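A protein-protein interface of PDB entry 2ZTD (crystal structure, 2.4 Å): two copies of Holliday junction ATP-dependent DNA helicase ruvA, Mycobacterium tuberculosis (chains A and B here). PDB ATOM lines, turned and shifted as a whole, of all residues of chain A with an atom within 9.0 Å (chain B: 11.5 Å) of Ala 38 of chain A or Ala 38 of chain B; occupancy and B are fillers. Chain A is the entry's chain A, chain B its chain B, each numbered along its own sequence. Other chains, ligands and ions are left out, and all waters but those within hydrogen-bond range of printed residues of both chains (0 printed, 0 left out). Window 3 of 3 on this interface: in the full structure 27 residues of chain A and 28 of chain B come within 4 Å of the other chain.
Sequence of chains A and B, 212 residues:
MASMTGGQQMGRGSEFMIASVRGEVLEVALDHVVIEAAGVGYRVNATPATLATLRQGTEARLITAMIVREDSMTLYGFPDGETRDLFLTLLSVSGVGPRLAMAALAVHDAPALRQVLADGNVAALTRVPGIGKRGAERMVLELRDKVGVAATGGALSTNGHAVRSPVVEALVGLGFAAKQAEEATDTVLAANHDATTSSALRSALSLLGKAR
The side-chain carboxylate (OE2) of Glu 36 of chain A is in salt-bridge range of the guanidinium group (NE) of Arg 22 of chain B, at 3.5 Å.
NH2 of Arg 61 of chain B is in salt-bridge range of OE1 of Glu 36 of chain A, 3.1 Å away.
The backbone NH of Arg 22 of chain B lies within hydrogen-bond range of the backbone carbonyl oxygen of Gly 39 of chain A, 2.9 Å away.
The backbone carbonyl oxygen of Gly 41 of chain A lies within hydrogen-bond range of the backbone NH of Ala 19 of chain B, at 2.7 Å.
N of Gly 41 of chain A lies within hydrogen-bond range of O of Ser 20 of chain B, at 3.0 Å.
O of Glu 24 of chain A is in hydrogen-bond range of N of Glu 36 of chain A (2.9 Å).
The backbone NH (N) of Leu 62 of chain B is in hydrogen-bond range of the backbone carbonyl oxygen (O) of Val 21 of chain B.
NH1 of Arg 22 of chain B lies within salt-bridge range of OE2 of Glu 59 of chain B (3.9 Å).
N of Ile 35 of chain B is in hydrogen-bond range of O of Tyr 42 of chain B (2.9 Å).
Among the printed residues, merely in contact across the chains: Ala 38 of chain A with Ala 37 of chain B (3.5 Å), Ala 38 of chain A with Ala 38 of chain B (3.7 Å), Gly 39 of chain A with Val 21 of chain B (3.7 Å), Val 40 of chain A with Ser 20 of chain B (3.9 Å), Val 40 of chain A with Tyr 42 of chain B (3.8 Å) and Gly 41 of chain A with Ile 18 of chain B (3.6 Å).
Of chain B, only Arg 22 (3.5 Å) and Arg 61 (3.1 Å) come within 4 Å of Glu 36 of chain A.
Gly 39 of chain A touches just these residues of chain B: Val 21 (3.7 Å) and Arg 22 (2.9 Å).
Val 40 of chain A touches just these residues of chain B: Ser 20 and Tyr 42.
Of the printed residues of chain A, Ser 20 of chain B touches Val 40 and Gly 41.
Printed residues of chain A within 4 Å of Val 21 of chain B: Gly 39.
Gly 23 of chain B touches none of the printed residues of chain A.
Of the printed residues of chain A, Ala 37 of chain B touches Ala 38 (3.5 Å).
Ala 38 of chain B touches one residue of chain A.
The nearest printed residue of chain A that does not touch Ser 20 of chain B is Gly 39 of chain A (4.1 Å).
Printed residues of chain A that touch a printed residue of chain B: Glu 36, Ala 38, Gly 39, Val 40 and Gly 41.
Printed residues of chain B that touch a printed residue of chain A: Ile 18, Ala 19, Ser 20, Val 21, Arg 22, Ala 37, Ala 38, Tyr 42 and Arg 61.
Hydrophobic or aromatic side chains of chain B within 4 Å of the printed part of chain A: Ala 19, Ala 37, Ala 38 and Tyr 42.
Glu 36 of chain A touches Arg 22 of chain B, but with the chains exchanged Arg 22 of chain A does not touch Glu 36 of chain B (15.5 Å).
Ala 38 of chain B touches its own counterpart, Ala 38 of chain A.
Gly 39 of chain A touches Arg 22 of chain B, but with the chains exchanged Arg 22 of chain A does not touch Gly 39 of chain B (14.8 Å).
Val 40 of chain A touches Tyr 42 of chain B, but with the chains exchanged Tyr 42 of chain A does not touch Val 40 of chain B (8.6 Å).
12 positions are printed for both chains.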
ATOM      1  N   VAL A  21      10.641  -6.978  -1.081  1.00  0.00           N
ATOM      2  CA  VAL A  21      10.322  -6.723   0.311  1.00  0.00           C
ATOM      3  C   VAL A  21       8.834  -7.003   0.527  1.00  0.00           C
ATOM      4  O   VAL A  21       7.997  -6.573  -0.259  1.00  0.00           O
ATOM      5  CB  VAL A  21      10.693  -5.275   0.755  1.00  0.00           C
ATOM      6  CG1 VAL A  21      10.369  -5.070   2.209  1.00  0.00           C
ATOM      7  CG2 VAL A  21      12.169  -4.984   0.522  1.00  0.00           C
ATOM      8  N   ARG A  22       8.523  -7.759   1.577  1.00  0.00           N
ATOM      9  CA  ARG A  22       7.137  -8.094   1.889  1.00  0.00           C
ATOM     10  C   ARG A  22       6.829  -7.858   3.362  1.00  0.00           C
ATOM     11  O   ARG A  22       7.675  -8.071   4.234  1.00  0.00           O
ATOM     12  CB  ARG A  22       6.850  -9.551   1.531  1.00  0.00           C
ATOM     13  CG  ARG A  22       5.494 -10.037   2.002  1.00  0.00           C
ATOM     14  CD  ARG A  22       5.389 -11.555   1.944  1.00  0.00           C
ATOM     15  NE  ARG A  22       5.984 -12.172   3.127  1.00  0.00           N
ATOM     16  CZ  ARG A  22       5.609 -13.337   3.637  1.00  0.00           C
ATOM     17  NH1 ARG A  22       4.630 -14.040   3.080  1.00  0.00           N
ATOM     18  NH2 ARG A  22       6.217 -13.801   4.717  1.00  0.00           N
ATOM     19  N   GLY A  23       5.615  -7.440   3.647  1.00  0.00           N
ATOM     20  CA  GLY A  23       5.207  -7.177   5.010  1.00  0.00           C
ATOM     21  C   GLY A  23       4.164  -6.075   5.030  1.00  0.00           C
ATOM     22  O   GLY A  23       3.546  -5.774   4.002  1.00  0.00           O
ATOM     23  N   GLU A  24       3.986  -5.458   6.193  1.00  0.00           N
ATOM     24  CA  GLU A  24       2.889  -4.502   6.380  1.00  0.00           C
ATOM     25  C   GLU A  24       3.138  -3.132   5.777  1.00  0.00           C
ATOM     26  O   GLU A  24       4.168  -2.511   6.053  1.00  0.00           O
ATOM     27  CB  GLU A  24       2.574  -4.334   7.859  1.00  0.00           C
ATOM     28  CG  GLU A  24       1.271  -3.624   8.120  1.00  0.00           C
ATOM     29  CD  GLU A  24       1.135  -3.232   9.576  1.00  0.00           C
ATOM     30  OE1 GLU A  24       1.962  -3.710  10.382  1.00  0.00           O
ATOM     31  OE2 GLU A  24       0.215  -2.447   9.910  1.00  0.00           O
ATOM     32  N   ILE A  35       7.299  -0.400   3.564  1.00  0.00           N
ATOM     33  CA  ILE A  35       6.859  -1.761   3.887  1.00  0.00           C
ATOM     34  C   ILE A  35       7.693  -2.342   5.020  1.00  0.00           C
ATOM     35  O   ILE A  35       8.922  -2.432   4.920  1.00  0.00           O
ATOM     36  CB  ILE A  35       6.902  -2.682   2.646  1.00  0.00           C
ATOM     37  CG1 ILE A  35       6.010  -2.111   1.527  1.00  0.00           C
ATOM     38  CG2 ILE A  35       6.474  -4.087   3.014  1.00  0.00           C
ATOM     39  CD1 ILE A  35       6.274  -2.703   0.169  1.00  0.00           C
ATOM     40  N   GLU A  36       7.022  -2.739   6.095  1.00  0.00           N
ATOM     41  CA  GLU A  36       7.717  -3.218   7.286  1.00  0.00           C
ATOM     42  C   GLU A  36       7.923  -4.735   7.283  1.00  0.00           C
ATOM     43  O   GLU A  36       6.965  -5.504   7.369  1.00  0.00           O
ATOM     44  CB  GLU A  36       7.006  -2.781   8.585  1.00  0.00           C
ATOM     45  CG  GLU A  36       7.811  -3.076   9.878  1.00  0.00           C
ATOM     46  CD  GLU A  36       7.106  -2.591  11.147  1.00  0.00           C
ATOM     47  OE1 GLU A  36       7.593  -1.620  11.778  1.00  0.00           O
ATOM     48  OE2 GLU A  36       6.067  -3.179  11.515  1.00  0.00           O
ATOM     49  N   ALA A  37       9.181  -5.138   7.183  1.00  0.00           N
ATOM     50  CA  ALA A  37       9.563  -6.538   7.283  1.00  0.00           C
ATOM     51  C   ALA A  37      10.421  -6.746   8.531  1.00  0.00           C
ATOM     52  O   ALA A  37      11.482  -6.126   8.674  1.00  0.00           O
ATOM     53  CB  ALA A  37      10.330  -6.967   6.022  1.00  0.00           C
ATOM     54  N   ALA A  38       9.970  -7.610   9.438  1.00  0.00           N
ATOM     55  CA  ALA A  38      10.770  -7.918  10.627  1.00  0.00           C
ATOM     56  C   ALA A  38      11.101  -6.641  11.400  1.00  0.00           C
ATOM     57  O   ALA A  38      12.256  -6.384  11.726  1.00  0.00           O
ATOM     58  CB  ALA A  38      12.068  -8.654  10.231  1.00  0.00           C
ATOM     59  N   GLY A  39      10.086  -5.828  11.659  1.00  0.00           N
ATOM     60  CA  GLY A  39      10.262  -4.587  12.390  1.00  0.00           C
ATOM     61  C   GLY A  39      11.048  -3.505  11.664  1.00  0.00           C
ATOM     62  O   GLY A  39      11.147  -2.380  12.178  1.00  0.00           O
ATOM     63  N   VAL A  40      11.625  -3.842  10.503  1.00  0.00           N
ATOM     64  CA  VAL A  40      12.352  -2.865   9.692  1.00  0.00           C
ATOM     65  C   VAL A  40      11.479  -2.270   8.577  1.00  0.00           C
ATOM     66  O   VAL A  40      10.898  -2.987   7.744  1.00  0.00           O
ATOM     67  CB  VAL A  40      13.654  -3.422   9.098  1.00  0.00           C
ATOM     68  CG1 VAL A  40      14.361  -2.343   8.299  1.00  0.00           C
ATOM     69  CG2 VAL A  40      14.561  -3.952  10.192  1.00  0.00           C
ATOM     70  N   GLY A  41      11.396  -0.946   8.566  1.00  0.00           N
ATOM     71  CA  GLY A  41      10.538  -0.273   7.611  1.00  0.00           C
ATOM     72  C   GLY A  41      11.341   0.150   6.409  1.00  0.00           C
ATOM     73  O   GLY A  41      12.168   1.064   6.497  1.00  0.00           O
ATOM     74  N   TYR A  42      11.098  -0.522   5.285  1.00  0.00           N
ATOM     75  CA  TYR A  42      11.844  -0.262   4.065  1.00  0.00           C
ATOM     76  C   TYR A  42      11.126   0.778   3.211  1.00  0.00           C
ATOM     77  O   TYR A  42       9.946   0.644   2.883  1.00  0.00           O
ATOM     78  CB  TYR A  42      12.097  -1.566   3.274  1.00  0.00           C
ATOM     79  CG  TYR A  42      13.054  -2.518   3.967  1.00  0.00           C
ATOM     80  CD1 TYR A  42      12.590  -3.539   4.790  1.00  0.00           C
ATOM     81  CD2 TYR A  42      14.426  -2.378   3.821  1.00  0.00           C
ATOM     82  CE1 TYR A  42      13.480  -4.405   5.449  1.00  0.00           C
ATOM     83  CE2 TYR A  42      15.311  -3.231   4.466  1.00  0.00           C
ATOM     84  CZ  TYR A  42      14.840  -4.239   5.281  1.00  0.00           C
ATOM     85  OH  TYR A  42      15.738  -5.071   5.905  1.00  0.00           O
ATOM     86  N   ILE B  18      16.266   2.510   4.991  1.00  0.00           N
ATOM     87  CA  ILE B  18      15.647   2.260   6.297  1.00  0.00           C
ATOM     88  C   ILE B  18      14.853   3.475   6.813  1.00  0.00           C
ATOM     89  O   ILE B  18      15.402   4.492   7.247  1.00  0.00           O
ATOM     90  CB  ILE B  18      16.630   1.738   7.357  1.00  0.00           C
ATOM     91  CG1 ILE B  18      17.364   0.504   6.831  1.00  0.00           C
ATOM     92  CG2 ILE B  18      15.874   1.382   8.640  1.00  0.00           C
ATOM     93  CD1 ILE B  18      18.147  -0.254   7.878  1.00  0.00           C
ATOM     94  N   ALA B  19      13.541   3.335   6.757  1.00  0.00           N
ATOM     95  CA  ALA B  19      12.646   4.449   6.985  1.00  0.00           C
ATOM     96  C   ALA B  19      12.123   4.453   8.410  1.00  0.00           C
ATOM     97  O   ALA B  19      11.607   5.468   8.872  1.00  0.00           O
ATOM     98  CB  ALA B  19      11.504   4.395   5.993  1.00  0.00           C
ATOM     99  N   SER B  20      12.256   3.321   9.087  1.00  0.00           N
ATOM    100  CA  SER B  20      11.950   3.208  10.515  1.00  0.00           C
ATOM    101  C   SER B  20      12.493   1.918  11.110  1.00  0.00           C
ATOM    102  O   SER B  20      12.757   0.944  10.392  1.00  0.00           O
ATOM    103  CB  SER B  20      10.428   3.297  10.749  1.00  0.00           C
ATOM    104  OG  SER B  20       9.744   2.184  10.203  1.00  0.00           O
ATOM    105  N   VAL B  21      12.656   1.908  12.428  1.00  0.00           N
ATOM    106  CA  VAL B  21      13.001   0.679  13.150  1.00  0.00           C
ATOM    107  C   VAL B  21      12.063   0.503  14.354  1.00  0.00           C
ATOM    108  O   VAL B  21      11.857   1.426  15.139  1.00  0.00           O
ATOM    109  CB  VAL B  21      14.489   0.653  13.588  1.00  0.00           C
ATOM    110  CG1 VAL B  21      14.816  -0.648  14.324  1.00  0.00           C
ATOM    111  CG2 VAL B  21      15.400   0.840  12.380  1.00  0.00           C
ATOM    112  N   ARG B  22      11.487  -0.688  14.482  1.00  0.00           N
ATOM    113  CA  ARG B  22      10.583  -0.987  15.582  1.00  0.00           C
ATOM    114  C   ARG B  22      10.952  -2.317  16.261  1.00  0.00           C
ATOM    115  O   ARG B  22      11.348  -3.279  15.610  1.00  0.00           O
ATOM    116  CB  ARG B  22       9.147  -1.040  15.079  1.00  0.00           C
ATOM    117  CG  ARG B  22       8.161  -1.518  16.127  1.00  0.00           C
ATOM    118  CD  ARG B  22       6.833  -1.940  15.523  1.00  0.00           C
ATOM    119  NE  ARG B  22       6.884  -3.289  14.962  1.00  0.00           N
ATOM    120  CZ  ARG B  22       5.840  -4.104  14.871  1.00  0.00           C
ATOM    121  NH1 ARG B  22       4.648  -3.707  15.313  1.00  0.00           N
ATOM    122  NH2 ARG B  22       5.981  -5.315  14.343  1.00  0.00           N
ATOM    123  N   GLY B  23      10.796  -2.362  17.570  1.00  0.00           N
ATOM    124  CA  GLY B  23      11.139  -3.548  18.326  1.00  0.00           C
ATOM    125  C   GLY B  23      11.525  -3.149  19.736  1.00  0.00           C
ATOM    126  O   GLY B  23      11.237  -2.031  20.171  1.00  0.00           O
ATOM    127  N   GLU B  24      12.199  -4.054  20.446  1.00  0.00           N
ATOM    128  CA  GLU B  24      12.465  -3.855  21.862  1.00  0.00           C
ATOM    129  C   GLU B  24      13.619  -2.899  22.136  1.00  0.00           C
ATOM    130  O   GLU B  24      14.710  -3.051  21.583  1.00  0.00           O
ATOM    131  CB  GLU B  24      12.740  -5.198  22.538  1.00  0.00           C
ATOM    132  CG  GLU B  24      12.754  -5.129  24.052  1.00  0.00           C
ATOM    133  CD  GLU B  24      13.348  -6.379  24.665  1.00  0.00           C
ATOM    134  OE1 GLU B  24      13.584  -7.345  23.913  1.00  0.00           O
ATOM    135  OE2 GLU B  24      13.571  -6.392  25.891  1.00  0.00           O
ATOM    136  N   VAL B  25      13.370  -1.909  22.991  1.00  0.00           N
ATOM    137  CA  VAL B  25      14.420  -1.005  23.421  1.00  0.00           C
ATOM    138  C   VAL B  25      15.341  -1.794  24.333  1.00  0.00           C
ATOM    139  O   VAL B  25      14.896  -2.334  25.346  1.00  0.00           O
ATOM    140  CB  VAL B  25      13.869   0.219  24.170  1.00  0.00           C
ATOM    141  CG1 VAL B  25      15.032   1.108  24.612  1.00  0.00           C
ATOM    142  CG2 VAL B  25      12.896   1.001  23.291  1.00  0.00           C
ATOM    143  N   LEU B  26      16.611  -1.876  23.958  1.00  0.00           N
ATOM    144  CA  LEU B  26      17.606  -2.624  24.718  1.00  0.00           C
ATOM    145  C   LEU B  26      18.516  -1.686  25.503  1.00  0.00           C
ATOM    146  O   LEU B  26      19.214  -2.095  26.427  1.00  0.00           O
ATOM    147  CB  LEU B  26      18.475  -3.471  23.778  1.00  0.00           C
ATOM    148  CG  LEU B  26      17.848  -4.571  22.918  1.00  0.00           C
ATOM    149  CD1 LEU B  26      18.941  -5.291  22.157  1.00  0.00           C
ATOM    150  CD2 LEU B  26      17.054  -5.555  23.737  1.00  0.00           C
ATOM    151  N   VAL B  34      19.240   1.734  21.388  1.00  0.00           N
ATOM    152  CA  VAL B  34      19.391   0.516  20.612  1.00  0.00           C
ATOM    153  C   VAL B  34      18.051  -0.187  20.540  1.00  0.00           C
ATOM    154  O   VAL B  34      17.490  -0.562  21.569  1.00  0.00           O
ATOM    155  CB  VAL B  34      20.465  -0.437  21.162  1.00  0.00           C
ATOM    156  CG1 VAL B  34      20.536  -1.654  20.254  1.00  0.00           C
ATOM    157  CG2 VAL B  34      21.834   0.249  21.222  1.00  0.00           C
ATOM    158  N   ILE B  35      17.517  -0.338  19.328  1.00  0.00           N
ATOM    159  CA  ILE B  35      16.219  -0.999  19.160  1.00  0.00           C
ATOM    160  C   ILE B  35      16.387  -2.316  18.411  1.00  0.00           C
ATOM    161  O   ILE B  35      16.882  -2.338  17.293  1.00  0.00           O
ATOM    162  CB  ILE B  35      15.199  -0.094  18.427  1.00  0.00           C
ATOM    163  CG1 ILE B  35      14.983   1.204  19.211  1.00  0.00           C
ATOM    164  CG2 ILE B  35      13.875  -0.831  18.243  1.00  0.00           C
ATOM    165  CD1 ILE B  35      14.311   2.332  18.395  1.00  0.00           C
ATOM    166  N   GLU B  36      15.998  -3.415  19.052  1.00  0.00           N
ATOM    167  CA  GLU B  36      16.202  -4.747  18.495  1.00  0.00           C
ATOM    168  C   GLU B  36      15.030  -5.224  17.634  1.00  0.00           C
ATOM    169  O   GLU B  36      13.938  -5.479  18.136  1.00  0.00           O
ATOM    170  CB  GLU B  36      16.503  -5.774  19.598  1.00  0.00           C
ATOM    171  CG  GLU B  36      16.910  -7.149  19.056  1.00  0.00           C
ATOM    172  CD  GLU B  36      17.222  -8.160  20.127  1.00  0.00           C
ATOM    173  OE1 GLU B  36      18.403  -8.539  20.263  1.00  0.00           O
ATOM    174  OE2 GLU B  36      16.295  -8.591  20.828  1.00  0.00           O
ATOM    175  N   ALA B  37      15.286  -5.350  16.336  1.00  0.00           N
ATOM    176  CA  ALA B  37      14.310  -5.879  15.385  1.00  0.00           C
ATOM    177  C   ALA B  37      14.842  -7.189  14.802  1.00  0.00           C
ATOM    178  O   ALA B  37      15.928  -7.225  14.216  1.00  0.00           O
ATOM    179  CB  ALA B  37      14.053  -4.872  14.277  1.00  0.00           C
ATOM    180  N   ALA B  38      14.095  -8.273  14.982  1.00  0.00           N
ATOM    181  CA  ALA B  38      14.510  -9.547  14.418  1.00  0.00           C
ATOM    182  C   ALA B  38      15.928  -9.918  14.887  1.00  0.00           C
ATOM    183  O   ALA B  38      16.794 -10.266  14.072  1.00  0.00           O
ATOM    184  CB  ALA B  38      14.454  -9.486  12.878  1.00  0.00           C
ATOM    185  N   GLY B  39      16.159  -9.821  16.191  1.00  0.00           N
ATOM    186  CA  GLY B  39      17.442 -10.197  16.753  1.00  0.00           C
ATOM    187  C   GLY B  39      18.583  -9.262  16.402  1.00  0.00           C
ATOM    188  O   GLY B  39      19.691  -9.411  16.926  1.00  0.00           O
ATOM    189  N   VAL B  40      18.332  -8.306  15.510  1.00  0.00           N
ATOM    190  CA  VAL B  40      19.345  -7.299  15.176  1.00  0.00           C
ATOM    191  C   VAL B  40      19.144  -5.980  15.960  1.00  0.00           C
ATOM    192  O   VAL B  40      18.071  -5.375  15.951  1.00  0.00           O
ATOM    193  CB  VAL B  40      19.353  -6.989  13.662  1.00  0.00           C
ATOM    194  CG1 VAL B  40      20.434  -5.955  13.334  1.00  0.00           C
ATOM    195  CG2 VAL B  40      19.570  -8.283  12.846  1.00  0.00           C
ATOM    196  N   GLY B  41      20.200  -5.555  16.648  1.00  0.00           N
ATOM    197  CA  GLY B  41      20.115  -4.386  17.497  1.00  0.00           C
ATOM    198  C   GLY B  41      20.603  -3.191  16.725  1.00  0.00           C
ATOM    199  O   GLY B  41      21.787  -3.080  16.412  1.00  0.00           O
ATOM    200  N   TYR B  42      19.679  -2.305  16.393  1.00  0.00           N
ATOM    201  CA  TYR B  42      20.001  -1.134  15.589  1.00  0.00           C
ATOM    202  C   TYR B  42      20.295   0.074  16.471  1.00  0.00           C
ATOM    203  O   TYR B  42      19.483   0.461  17.320  1.00  0.00           O
ATOM    204  CB  TYR B  42      18.859  -0.801  14.615  1.00  0.00           C
ATOM    205  CG  TYR B  42      18.690  -1.802  13.505  1.00  0.00           C
ATOM    206  CD1 TYR B  42      17.766  -2.832  13.602  1.00  0.00           C
ATOM    207  CD2 TYR B  42      19.463  -1.724  12.358  1.00  0.00           C
ATOM    208  CE1 TYR B  42      17.615  -3.760  12.569  1.00  0.00           C
ATOM    209  CE2 TYR B  42      19.320  -2.645  11.330  1.00  0.00           C
ATOM    210  CZ  TYR B  42      18.397  -3.657  11.438  1.00  0.00           C
ATOM    211  OH  TYR B  42      18.266  -4.556  10.406  1.00  0.00           O
ATOM    212  N   GLU B  59       8.644  -2.005  23.756  1.00  0.00           N
ATOM    213  CA  GLU B  59       8.720  -1.899  22.314  1.00  0.00           C
ATOM    214  C   GLU B  59       8.593  -0.447  21.901  1.00  0.00           C
ATOM    215  O   GLU B  59       7.808   0.305  22.475  1.00  0.00           O
ATOM    216  CB  GLU B  59       7.623  -2.725  21.663  1.00  0.00           C
ATOM    217  CG  GLU B  59       7.765  -2.822  20.160  1.00  0.00           C
ATOM    218  CD  GLU B  59       6.543  -3.417  19.511  1.00  0.00           C
ATOM    219  OE1 GLU B  59       6.314  -4.634  19.662  1.00  0.00           O
ATOM    220  OE2 GLU B  59       5.805  -2.653  18.846  1.00  0.00           O
ATOM    221  N   ALA B  60       9.384  -0.045  20.912  1.00  0.00           N
ATOM    222  CA  ALA B  60       9.301   1.311  20.378  1.00  0.00           C
ATOM    223  C   ALA B  60       9.462   1.319  18.865  1.00  0.00           C
ATOM    224  O   ALA B  60       9.897   0.335  18.256  1.00  0.00           O
ATOM    225  CB  ALA B  60      10.346   2.225  21.031  1.00  0.00           C
ATOM    226  N   ARG B  61       9.101   2.437  18.268  1.00  0.00           N
ATOM    227  CA  ARG B  61       9.300   2.639  16.840  1.00  0.00           C
ATOM    228  C   ARG B  61       9.766   4.058  16.600  1.00  0.00           C
ATOM    229  O   ARG B  61       9.121   5.007  17.020  1.00  0.00           O
ATOM    230  CB  ARG B  61       8.013   2.371  16.053  1.00  0.00           C
ATOM    231  CG  ARG B  61       8.084   2.882  14.611  1.00  0.00           C
ATOM    232  CD  ARG B  61       6.726   2.793  13.925  1.00  0.00           C
ATOM    233  NE  ARG B  61       6.424   1.433  13.488  1.00  0.00           N
ATOM    234  CZ  ARG B  61       5.204   0.926  13.371  1.00  0.00           C
ATOM    235  NH1 ARG B  61       4.141   1.674  13.668  1.00  0.00           N
ATOM    236  NH2 ARG B  61       5.045  -0.332  12.964  1.00  0.00           N
ATOM    237  N   LEU B  62      10.891   4.204  15.925  1.00  0.00           N
ATOM    238  CA  LEU B  62      11.356   5.519  15.531  1.00  0.00           C
ATOM    239  C   LEU B  62      11.350   5.601  14.020  1.00  0.00           C
ATOM    240  O   LEU B  62      11.580   4.604  13.356  1.00  0.00           O
ATOM    241  CB  LEU B  62      12.768   5.774  16.078  1.00  0.00           C
ATOM    242  CG  LEU B  62      12.894   6.298  17.514  1.00  0.00           C
ATOM    243  CD1 LEU B  62      14.353   6.251  17.980  1.00  0.00           C
ATOM    244  CD2 LEU B  62      12.329   7.722  17.601  1.00  0.00           C
ATOM    245  N   LEU B  75      21.940   5.472  11.308  1.00  0.00           N
ATOM    246  CA  LEU B  75      20.528   5.769  11.439  1.00  0.00           C
ATOM    247  C   LEU B  75      20.322   6.922  12.410  1.00  0.00           C
ATOM    248  O   LEU B  75      20.877   6.918  13.532  1.00  0.00           O
ATOM    249  CB  LEU B  75      19.754   4.535  11.915  1.00  0.00           C
ATOM    250  CG  LEU B  75      19.701   3.367  10.915  1.00  0.00           C
ATOM    251  CD1 LEU B  75      19.211   2.083  11.558  1.00  0.00           C
ATOM    252  CD2 LEU B  75      18.824   3.711   9.726  1.00  0.00           C
